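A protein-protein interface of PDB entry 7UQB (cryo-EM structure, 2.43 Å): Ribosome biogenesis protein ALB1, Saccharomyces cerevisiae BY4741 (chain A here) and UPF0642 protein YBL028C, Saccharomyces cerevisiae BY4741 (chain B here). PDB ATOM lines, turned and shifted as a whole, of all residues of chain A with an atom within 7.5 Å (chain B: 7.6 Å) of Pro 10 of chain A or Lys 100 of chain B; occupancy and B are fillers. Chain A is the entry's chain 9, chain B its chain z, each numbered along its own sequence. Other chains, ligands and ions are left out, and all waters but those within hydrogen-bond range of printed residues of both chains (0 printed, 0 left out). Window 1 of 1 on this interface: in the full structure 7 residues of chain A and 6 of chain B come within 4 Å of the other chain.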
ATOM      1  N   PRO A   2     -21.353  26.191  20.743  1.00  0.00           N
ATOM      2  CA  PRO A   2     -21.573  25.254  21.848  1.00  0.00           C
ATOM      3  C   PRO A   2     -21.882  25.960  23.164  1.00  0.00           C
ATOM      4  O   PRO A   2     -21.500  27.112  23.353  1.00  0.00           O
ATOM      5  CB  PRO A   2     -20.244  24.504  21.934  1.00  0.00           C
ATOM      6  CG  PRO A   2     -19.241  25.499  21.469  1.00  0.00           C
ATOM      7  CD  PRO A   2     -19.925  26.315  20.403  1.00  0.00           C
ATOM      8  N   SER A   3     -22.579  25.267  24.059  1.00  0.00           N
ATOM      9  CA  SER A   3     -22.890  25.826  25.366  1.00  0.00           C
ATOM     10  C   SER A   3     -21.659  25.811  26.266  1.00  0.00           C
ATOM     11  O   SER A   3     -20.792  24.941  26.155  1.00  0.00           O
ATOM     12  CB  SER A   3     -24.027  25.045  26.020  1.00  0.00           C
ATOM     13  OG  SER A   3     -24.237  25.462  27.356  1.00  0.00           O
ATOM     14  N   SER A   6     -21.253  22.622  28.237  1.00  0.00           N
ATOM     15  CA  SER A   6     -20.746  21.442  27.532  1.00  0.00           C
ATOM     16  C   SER A   6     -20.115  21.924  26.224  1.00  0.00           C
ATOM     17  O   SER A   6     -20.791  22.031  25.199  1.00  0.00           O
ATOM     18  CB  SER A   6     -21.859  20.433  27.287  1.00  0.00           C
ATOM     19  OG  SER A   6     -22.990  21.052  26.702  1.00  0.00           O
ATOM     20  N   ILE A   7     -18.808  22.187  26.266  1.00  0.00           N
ATOM     21  CA  ILE A   7     -18.147  22.760  25.099  1.00  0.00           C
ATOM     22  C   ILE A   7     -17.809  21.719  24.040  1.00  0.00           C
ATOM     23  O   ILE A   7     -17.602  22.085  22.878  1.00  0.00           O
ATOM     24  CB  ILE A   7     -16.864  23.516  25.487  1.00  0.00           C
ATOM     25  CG1 ILE A   7     -15.939  22.619  26.312  1.00  0.00           C
ATOM     26  CG2 ILE A   7     -17.204  24.806  26.220  1.00  0.00           C
ATOM     27  CD1 ILE A   7     -14.484  22.998  26.215  1.00  0.00           C
ATOM     28  N   ASN A   8     -17.745  20.440  24.398  1.00  0.00           N
ATOM     29  CA  ASN A   8     -17.368  19.399  23.451  1.00  0.00           C
ATOM     30  C   ASN A   8     -18.552  18.814  22.692  1.00  0.00           C
ATOM     31  O   ASN A   8     -18.343  17.998  21.791  1.00  0.00           O
ATOM     32  CB  ASN A   8     -16.614  18.279  24.173  1.00  0.00           C
ATOM     33  CG  ASN A   8     -15.238  18.711  24.637  1.00  0.00           C
ATOM     34  OD1 ASN A   8     -14.690  19.698  24.153  1.00  0.00           O
ATOM     35  ND2 ASN A   8     -14.669  17.967  25.575  1.00  0.00           N
ATOM     36  N   ARG A   9     -19.782  19.209  23.021  1.00  0.00           N
ATOM     37  CA  ARG A   9     -20.954  18.704  22.325  1.00  0.00           C
ATOM     38  C   ARG A   9     -21.447  19.744  21.334  1.00  0.00           C
ATOM     39  O   ARG A   9     -21.710  20.888  21.735  1.00  0.00           O
ATOM     40  CB  ARG A   9     -22.062  18.349  23.308  1.00  0.00           C
ATOM     41  CG  ARG A   9     -23.262  17.681  22.656  1.00  0.00           C
ATOM     42  CD  ARG A   9     -24.251  17.167  23.685  1.00  0.00           C
ATOM     43  NE  ARG A   9     -24.864  18.247  24.447  1.00  0.00           N
ATOM     44  CZ  ARG A   9     -25.623  18.066  25.519  1.00  0.00           C
ATOM     45  NH1 ARG A   9     -25.879  16.858  25.989  1.00  0.00           N
ATOM     46  NH2 ARG A   9     -26.131  19.127  26.140  1.00  0.00           N
ATOM     47  N   PRO A  10     -21.574  19.411  20.050  1.00  0.00           N
ATOM     48  CA  PRO A  10     -22.098  20.386  19.086  1.00  0.00           C
ATOM     49  C   PRO A  10     -23.561  20.701  19.358  1.00  0.00           C
ATOM     50  O   PRO A  10     -24.366  19.813  19.647  1.00  0.00           O
ATOM     51  CB  PRO A  10     -21.917  19.683  17.735  1.00  0.00           C
ATOM     52  CG  PRO A  10     -20.935  18.576  17.995  1.00  0.00           C
ATOM     53  CD  PRO A  10     -21.185  18.151  19.400  1.00  0.00           C
ATOM     54  N   LYS A  11     -23.896  21.987  19.275  1.00  0.00           N
ATOM     55  CA  LYS A  11     -25.246  22.460  19.553  1.00  0.00           C
ATOM     56  C   LYS A  11     -25.892  23.097  18.330  1.00  0.00           C
ATOM     57  O   LYS A  11     -26.963  22.652  17.895  1.00  0.00           O
ATOM     58  CB  LYS A  11     -25.187  23.445  20.729  1.00  0.00           C
ATOM     59  CG  LYS A  11     -26.519  23.900  21.271  1.00  0.00           C
ATOM     60  CD  LYS A  11     -26.302  24.821  22.457  1.00  0.00           C
ATOM     61  CE  LYS A  11     -27.609  25.326  23.021  1.00  0.00           C
ATOM     62  NZ  LYS A  11     -28.505  24.213  23.429  1.00  0.00           N
ATOM     63  N   LEU A  12     -25.252  24.117  17.749  1.00  0.00           N
ATOM     64  CA  LEU A  12     -25.812  24.798  16.586  1.00  0.00           C
ATOM     65  C   LEU A  12     -25.910  23.867  15.386  1.00  0.00           C
ATOM     66  O   LEU A  12     -26.917  23.872  14.671  1.00  0.00           O
ATOM     67  CB  LEU A  12     -24.964  26.021  16.236  1.00  0.00           C
ATOM     68  CG  LEU A  12     -25.377  26.785  14.975  1.00  0.00           C
ATOM     69  CD1 LEU A  12     -26.622  27.617  15.230  1.00  0.00           C
ATOM     70  CD2 LEU A  12     -24.244  27.650  14.456  1.00  0.00           C
ATOM     71  N   THR A  13     -24.870  23.064  15.144  1.00  0.00           N
ATOM     72  CA  THR A  13     -24.876  22.178  13.983  1.00  0.00           C
ATOM     73  C   THR A  13     -25.936  21.091  14.115  1.00  0.00           C
ATOM     74  O   THR A  13     -26.608  20.756  13.135  1.00  0.00           O
ATOM     75  CB  THR A  13     -23.493  21.562  13.781  1.00  0.00           C
ATOM     76  OG1 THR A  13     -22.991  21.082  15.032  1.00  0.00           O
ATOM     77  CG2 THR A  13     -22.534  22.595  13.219  1.00  0.00           C
ATOM     78  N   SER A  14     -26.112  20.541  15.319  1.00  0.00           N
ATOM     79  CA  SER A  14     -27.163  19.551  15.531  1.00  0.00           C
ATOM     80  C   SER A  14     -28.548  20.164  15.353  1.00  0.00           C
ATOM     81  O   SER A  14     -29.435  19.546  14.745  1.00  0.00           O
ATOM     82  CB  SER A  14     -27.020  18.921  16.915  1.00  0.00           C
ATOM     83  OG  SER A  14     -27.089  19.899  17.935  1.00  0.00           O
ATOM     84  N   ASN A  15     -28.752  21.383  15.867  1.00  0.00           N
ATOM     85  CA  ASN A  15     -30.040  22.048  15.683  1.00  0.00           C
ATOM     86  C   ASN A  15     -30.324  22.320  14.209  1.00  0.00           C
ATOM     87  O   ASN A  15     -31.445  22.099  13.736  1.00  0.00           O
ATOM     88  CB  ASN A  15     -30.085  23.346  16.490  1.00  0.00           C
ATOM     89  CG  ASN A  15     -30.122  23.101  17.986  1.00  0.00           C
ATOM     90  OD1 ASN A  15     -30.550  22.044  18.443  1.00  0.00           O
ATOM     91  ND2 ASN A  15     -29.679  24.086  18.757  1.00  0.00           N
ATOM     92  N   HIS A  17     -29.082  20.670  11.620  1.00  0.00           N
ATOM     93  CA  HIS A  17     -29.305  19.391  10.953  1.00  0.00           C
ATOM     94  C   HIS A  17     -30.728  18.894  11.179  1.00  0.00           C
ATOM     95  O   HIS A  17     -31.410  18.474  10.231  1.00  0.00           O
ATOM     96  CB  HIS A  17     -28.284  18.371  11.458  1.00  0.00           C
ATOM     97  CG  HIS A  17     -28.135  17.172  10.576  1.00  0.00           C
ATOM     98  ND1 HIS A  17     -28.773  15.978  10.831  1.00  0.00           N
ATOM     99  CD2 HIS A  17     -27.415  16.982   9.447  1.00  0.00           C
ATOM    100  CE1 HIS A  17     -28.457  15.105   9.892  1.00  0.00           C
ATOM    101  NE2 HIS A  17     -27.634  15.689   9.040  1.00  0.00           N
ATOM    102  N   HIS A  18     -31.203  18.973  12.426  1.00  0.00           N
ATOM    103  CA  HIS A  18     -32.574  18.578  12.730  1.00  0.00           C
ATOM    104  C   HIS A  18     -33.583  19.453  11.995  1.00  0.00           C
ATOM    105  O   HIS A  18     -34.583  18.950  11.469  1.00  0.00           O
ATOM    106  CB  HIS A  18     -32.808  18.640  14.240  1.00  0.00           C
ATOM    107  CG  HIS A  18     -34.225  18.378  14.645  1.00  0.00           C
ATOM    108  ND1 HIS A  18     -34.744  17.106  14.758  1.00  0.00           N
ATOM    109  CD2 HIS A  18     -35.231  19.224  14.971  1.00  0.00           C
ATOM    110  CE1 HIS A  18     -36.008  17.181  15.133  1.00  0.00           C
ATOM    111  NE2 HIS A  18     -36.328  18.455  15.269  1.00  0.00           N
ATOM    112  N   MET B  94     -25.845   5.195  18.678  1.00  0.00           N
ATOM    113  CA  MET B  94     -26.271   5.452  17.306  1.00  0.00           C
ATOM    114  C   MET B  94     -27.085   6.736  17.215  1.00  0.00           C
ATOM    115  O   MET B  94     -26.938   7.504  16.258  1.00  0.00           O
ATOM    116  CB  MET B  94     -27.075   4.265  16.777  1.00  0.00           C
ATOM    117  CG  MET B  94     -27.424   4.370  15.308  1.00  0.00           C
ATOM    118  SD  MET B  94     -25.951   4.485  14.278  1.00  0.00           S
ATOM    119  CE  MET B  94     -25.156   2.927  14.664  1.00  0.00           C
ATOM    120  N   LYS B  95     -27.949   6.985  18.203  1.00  0.00           N
ATOM    121  CA  LYS B  95     -28.730   8.217  18.221  1.00  0.00           C
ATOM    122  C   LYS B  95     -27.831   9.440  18.340  1.00  0.00           C
ATOM    123  O   LYS B  95     -28.053  10.447  17.660  1.00  0.00           O
ATOM    124  CB  LYS B  95     -29.738   8.177  19.369  1.00  0.00           C
ATOM    125  CG  LYS B  95     -30.524   9.461  19.556  1.00  0.00           C
ATOM    126  CD  LYS B  95     -31.365   9.424  20.821  1.00  0.00           C
ATOM    127  CE  LYS B  95     -32.439   8.353  20.745  1.00  0.00           C
ATOM    128  NZ  LYS B  95     -33.346   8.393  21.927  1.00  0.00           N
ATOM    129  N   GLN B  96     -26.811   9.371  19.202  1.00  0.00           N
ATOM    130  CA  GLN B  96     -25.876  10.487  19.327  1.00  0.00           C
ATOM    131  C   GLN B  96     -25.094  10.705  18.036  1.00  0.00           C
ATOM    132  O   GLN B  96     -24.885  11.849  17.615  1.00  0.00           O
ATOM    133  CB  GLN B  96     -24.922  10.250  20.497  1.00  0.00           C
ATOM    134  CG  GLN B  96     -25.565  10.408  21.857  1.00  0.00           C
ATOM    135  CD  GLN B  96     -24.588  10.194  22.992  1.00  0.00           C
ATOM    136  OE1 GLN B  96     -23.376  10.189  22.791  1.00  0.00           O
ATOM    137  NE2 GLN B  96     -25.114  10.009  24.197  1.00  0.00           N
ATOM    138  N   SER B  97     -24.664   9.618  17.392  1.00  0.00           N
ATOM    139  CA  SER B  97     -23.928   9.735  16.136  1.00  0.00           C
ATOM    140  C   SER B  97     -24.796  10.334  15.035  1.00  0.00           C
ATOM    141  O   SER B  97     -24.315  11.132  14.221  1.00  0.00           O
ATOM    142  CB  SER B  97     -23.396   8.367  15.713  1.00  0.00           C
ATOM    143  OG  SER B  97     -22.714   8.442  14.475  1.00  0.00           O
ATOM    144  N   LYS B  98     -26.075   9.957  14.989  1.00  0.00           N
ATOM    145  CA  LYS B  98     -26.962  10.442  13.938  1.00  0.00           C
ATOM    146  C   LYS B  98     -27.403  11.882  14.179  1.00  0.00           C
ATOM    147  O   LYS B  98     -27.499  12.669  13.232  1.00  0.00           O
ATOM    148  CB  LYS B  98     -28.178   9.525  13.818  1.00  0.00           C
ATOM    149  CG  LYS B  98     -29.071   9.827  12.629  1.00  0.00           C
ATOM    150  CD  LYS B  98     -28.294   9.733  11.324  1.00  0.00           C
ATOM    151  CE  LYS B  98     -29.176  10.069  10.132  1.00  0.00           C
ATOM    152  NZ  LYS B  98     -29.798  11.418  10.270  1.00  0.00           N
ATOM    153  N   LYS B  99     -27.675  12.248  15.430  1.00  0.00           N
ATOM    154  CA  LYS B  99     -28.122  13.594  15.759  1.00  0.00           C
ATOM    155  C   LYS B  99     -26.974  14.551  16.045  1.00  0.00           C
ATOM    156  O   LYS B  99     -27.235  15.714  16.369  1.00  0.00           O
ATOM    157  CB  LYS B  99     -29.068  13.560  16.964  1.00  0.00           C
ATOM    158  CG  LYS B  99     -30.481  13.102  16.640  1.00  0.00           C
ATOM    159  CD  LYS B  99     -31.310  12.978  17.909  1.00  0.00           C
ATOM    160  CE  LYS B  99     -32.799  12.925  17.605  1.00  0.00           C
ATOM    161  NZ  LYS B  99     -33.295  14.215  17.055  1.00  0.00           N
ATOM    162  N   LYS B 100     -25.723  14.086  15.941  1.00  0.00           N
ATOM    163  CA  LYS B 100     -24.533  14.923  16.120  1.00  0.00           C
ATOM    164  C   LYS B 100     -24.501  15.563  17.508  1.00  0.00           C
ATOM    165  O   LYS B 100     -24.146  16.732  17.667  1.00  0.00           O
ATOM    166  CB  LYS B 100     -24.433  15.989  15.024  1.00  0.00           C
ATOM    167  CG  LYS B 100     -24.325  15.421  13.615  1.00  0.00           C
ATOM    168  CD  LYS B 100     -24.506  16.504  12.565  1.00  0.00           C
ATOM    169  CE  LYS B 100     -24.309  15.954  11.162  1.00  0.00           C
ATOM    170  NZ  LYS B 100     -25.242  14.834  10.862  1.00  0.00           N
ATOM    171  N   THR B 101     -24.877  14.788  18.521  1.00  0.00           N
ATOM    172  CA  THR B 101     -24.873  15.225  19.910  1.00  0.00           C
ATOM    173  C   THR B 101     -23.930  14.370  20.748  1.00  0.00           C
ATOM    174  O   THR B 101     -24.236  14.000  21.882  1.00  0.00           O
ATOM    175  CB  THR B 101     -26.282  15.199  20.497  1.00  0.00           C
ATOM    176  OG1 THR B 101     -26.893  13.931  20.225  1.00  0.00           O
ATOM    177  CG2 THR B 101     -27.133  16.307  19.898  1.00  0.00           C
ATOM    178  N   SER B 102     -22.767  14.044  20.195  1.00  0.00           N
ATOM    179  CA  SER B 102     -21.766  13.266  20.907  1.00  0.00           C
ATOM    180  C   SER B 102     -20.751  14.184  21.577  1.00  0.00           C
ATOM    181  O   SER B 102     -20.459  15.279  21.091  1.00  0.00           O
ATOM    182  CB  SER B 102     -21.048  12.304  19.959  1.00  0.00           C
ATOM    183  OG  SER B 102     -20.113  11.505  20.661  1.00  0.00           O
ATOM    184  N   PHE B 103     -20.212  13.720  22.704  1.00  0.00           N
ATOM    185  CA  PHE B 103     -19.230  14.486  23.458  1.00  0.00           C
ATOM    186  C   PHE B 103     -17.795  14.201  23.040  1.00  0.00           C
ATOM    187  O   PHE B 103     -16.950  15.099  23.115  1.00  0.00           O
ATOM    188  CB  PHE B 103     -19.372  14.204  24.956  1.00  0.00           C
ATOM    189  CG  PHE B 103     -20.442  15.010  25.627  1.00  0.00           C
ATOM    190  CD1 PHE B 103     -21.742  14.536  25.707  1.00  0.00           C
ATOM    191  CD2 PHE B 103     -20.148  16.242  26.182  1.00  0.00           C
ATOM    192  CE1 PHE B 103     -22.727  15.279  26.326  1.00  0.00           C
ATOM    193  CE2 PHE B 103     -21.129  16.988  26.805  1.00  0.00           C
ATOM    194  CZ  PHE B 103     -22.420  16.507  26.876  1.00  0.00           C
ATOM    195  N   THR B 104     -17.495  12.978  22.607  1.00  0.00           N
ATOM    196  CA  THR B 104     -16.128  12.583  22.315  1.00  0.00           C
ATOM    197  C   THR B 104     -15.881  12.202  20.865  1.00  0.00           C
ATOM    198  O   THR B 104     -14.716  12.096  20.469  1.00  0.00           O
ATOM    199  CB  THR B 104     -15.709  11.398  23.200  1.00  0.00           C
ATOM    200  OG1 THR B 104     -16.618  10.309  23.005  1.00  0.00           O
ATOM    201  CG2 THR B 104     -15.710  11.800  24.661  1.00  0.00           C
ATOM    202  N   ARG B 105     -16.919  11.992  20.067  1.00  0.00           N
ATOM    203  CA  ARG B 105     -16.762  11.478  18.717  1.00  0.00           C
ATOM    204  C   ARG B 105     -17.386  12.434  17.713  1.00  0.00           C
ATOM    205  O   ARG B 105     -18.460  12.992  17.955  1.00  0.00           O
ATOM    206  CB  ARG B 105     -17.387  10.088  18.592  1.00  0.00           C
ATOM    207  CG  ARG B 105     -16.795   9.088  19.564  1.00  0.00           C
ATOM    208  CD  ARG B 105     -17.540   7.770  19.564  1.00  0.00           C
ATOM    209  NE  ARG B 105     -17.022   6.873  20.590  1.00  0.00           N
ATOM    210  CZ  ARG B 105     -16.004   6.042  20.412  1.00  0.00           C
ATOM    211  NH1 ARG B 105     -15.382   5.949  19.249  1.00  0.00           N
ATOM    212  NH2 ARG B 105     -15.598   5.288  21.430  1.00  0.00           N
ATOM    213  N   PHE B 106     -16.694  12.633  16.597  1.00  0.00           N
ATOM    214  CA  PHE B 106     -17.219  13.430  15.499  1.00  0.00           C
ATOM    215  C   PHE B 106     -17.994  12.539  14.538  1.00  0.00           C
ATOM    216  O   PHE B 106     -17.784  11.326  14.497  1.00  0.00           O
ATOM    217  CB  PHE B 106     -16.093  14.155  14.757  1.00  0.00           C
ATOM    218  CG  PHE B 106     -15.606  15.398  15.449  1.00  0.00           C
ATOM    219  CD1 PHE B 106     -16.451  16.478  15.634  1.00  0.00           C
ATOM    220  CD2 PHE B 106     -14.301  15.492  15.899  1.00  0.00           C
ATOM    221  CE1 PHE B 106     -16.004  17.626  16.263  1.00  0.00           C
ATOM    222  CE2 PHE B 106     -13.850  16.636  16.528  1.00  0.00           C
ATOM    223  CZ  PHE B 106     -14.703  17.703  16.712  1.00  0.00           C
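Leu 12 of chain A touches none of the printed residues of chain B.
Thr 13 of chain A touches none of the printed residues of chain B.
Printed residues of chain B within 4 Å of His 17 of chain A: Lys 98 (3.9 Å) and Lys 100 (3.1 Å).
Lys 100 of chain B touches just these residues of chain A: Pro 10 (3.7 Å), Ser 14 (3.7 Å) and His 17 (3.1 Å).
Printed residues of chain A within 4 Å of Ser 102 of chain B: Asn 8, Arg 9 and Pro 10.
The nearest residue of chain B that does not touch Pro 10 of chain A is Thr 101 of chain B (4.5 Å).
The nearest printed residue of chain A that does not touch Thr 101 of chain B is Pro 10 of chain A (4.5 Å).
The backbone carbonyl oxygen (O) of Asn 8 of chain A lies close to the backbone carbonyl oxygen (O) of Phe 103 of chain B, at 3.5 Å.
NZ of Lys 100 of chain B is in hydrogen-bond range of NE2 of His 17 of chain A, at 3.1 Å.
Hydrophobic or aromatic side chains of chain B within 4 Å of the printed part of chain A: Phe 103.
Of the 14 printed residues of chain A, 7 touch a printed residue of chain B.
Printed residues of chain A that touch a printed residue of chain B: Ser 6, Asn 8, Arg 9, Pro 10, Ser 14, His 17 and His 18.
Hydrophobic or aromatic side chains of chain A that line the printed part of chain B: Pro 10, His 17 and His 18.
Along chain A the printed residues that touch a printed residue of chain B span positions 6 to 18.
Among the printed residues, pairs that only touch across the chains: Ser 6 of chain A with Phe 103 of chain B, Asn 8 of chain A with Ser 102 of chain B, Arg 9 of chain A with Thr 101 of chain B, Arg 9 of chain A with Ser 102 of chain B, Arg 9 of chain A with Phe 103 of chain B, Pro 10 of chain A with Lys 100 of chain B, Pro 10 of chain A with Ser 102 of chain B, Ser 14 of chain A with Lys 99 of chain B, Ser 14 of chain A with Lys 100 of chain B, Ser 14 of chain A with Thr 101 of chain B, His 17 of chain A with Lys 98 of chain B and His 18 of chain A with Lys 99 of chain B.
The backbone carbonyl oxygen of Lys 11 of chain A sits at hydrogen-bond distance from the side-chain hydroxyl of Ser 14 of chain A.
The backbone carbonyl oxygen of Pro 10 of chain A sits at hydrogen-bond distance from the side-chain hydroxyl of Ser 14 of chain A (3.2 Å).
N of Arg 105 of chain B sits at hydrogen-bond distance from OG of Ser 102 of chain B (3.3 Å).
The backbone carbonyl oxygen (O) of Gln 96 of chain B lies within hydrogen-bond range of the backbone NH (N) of Thr 101 of chain B.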
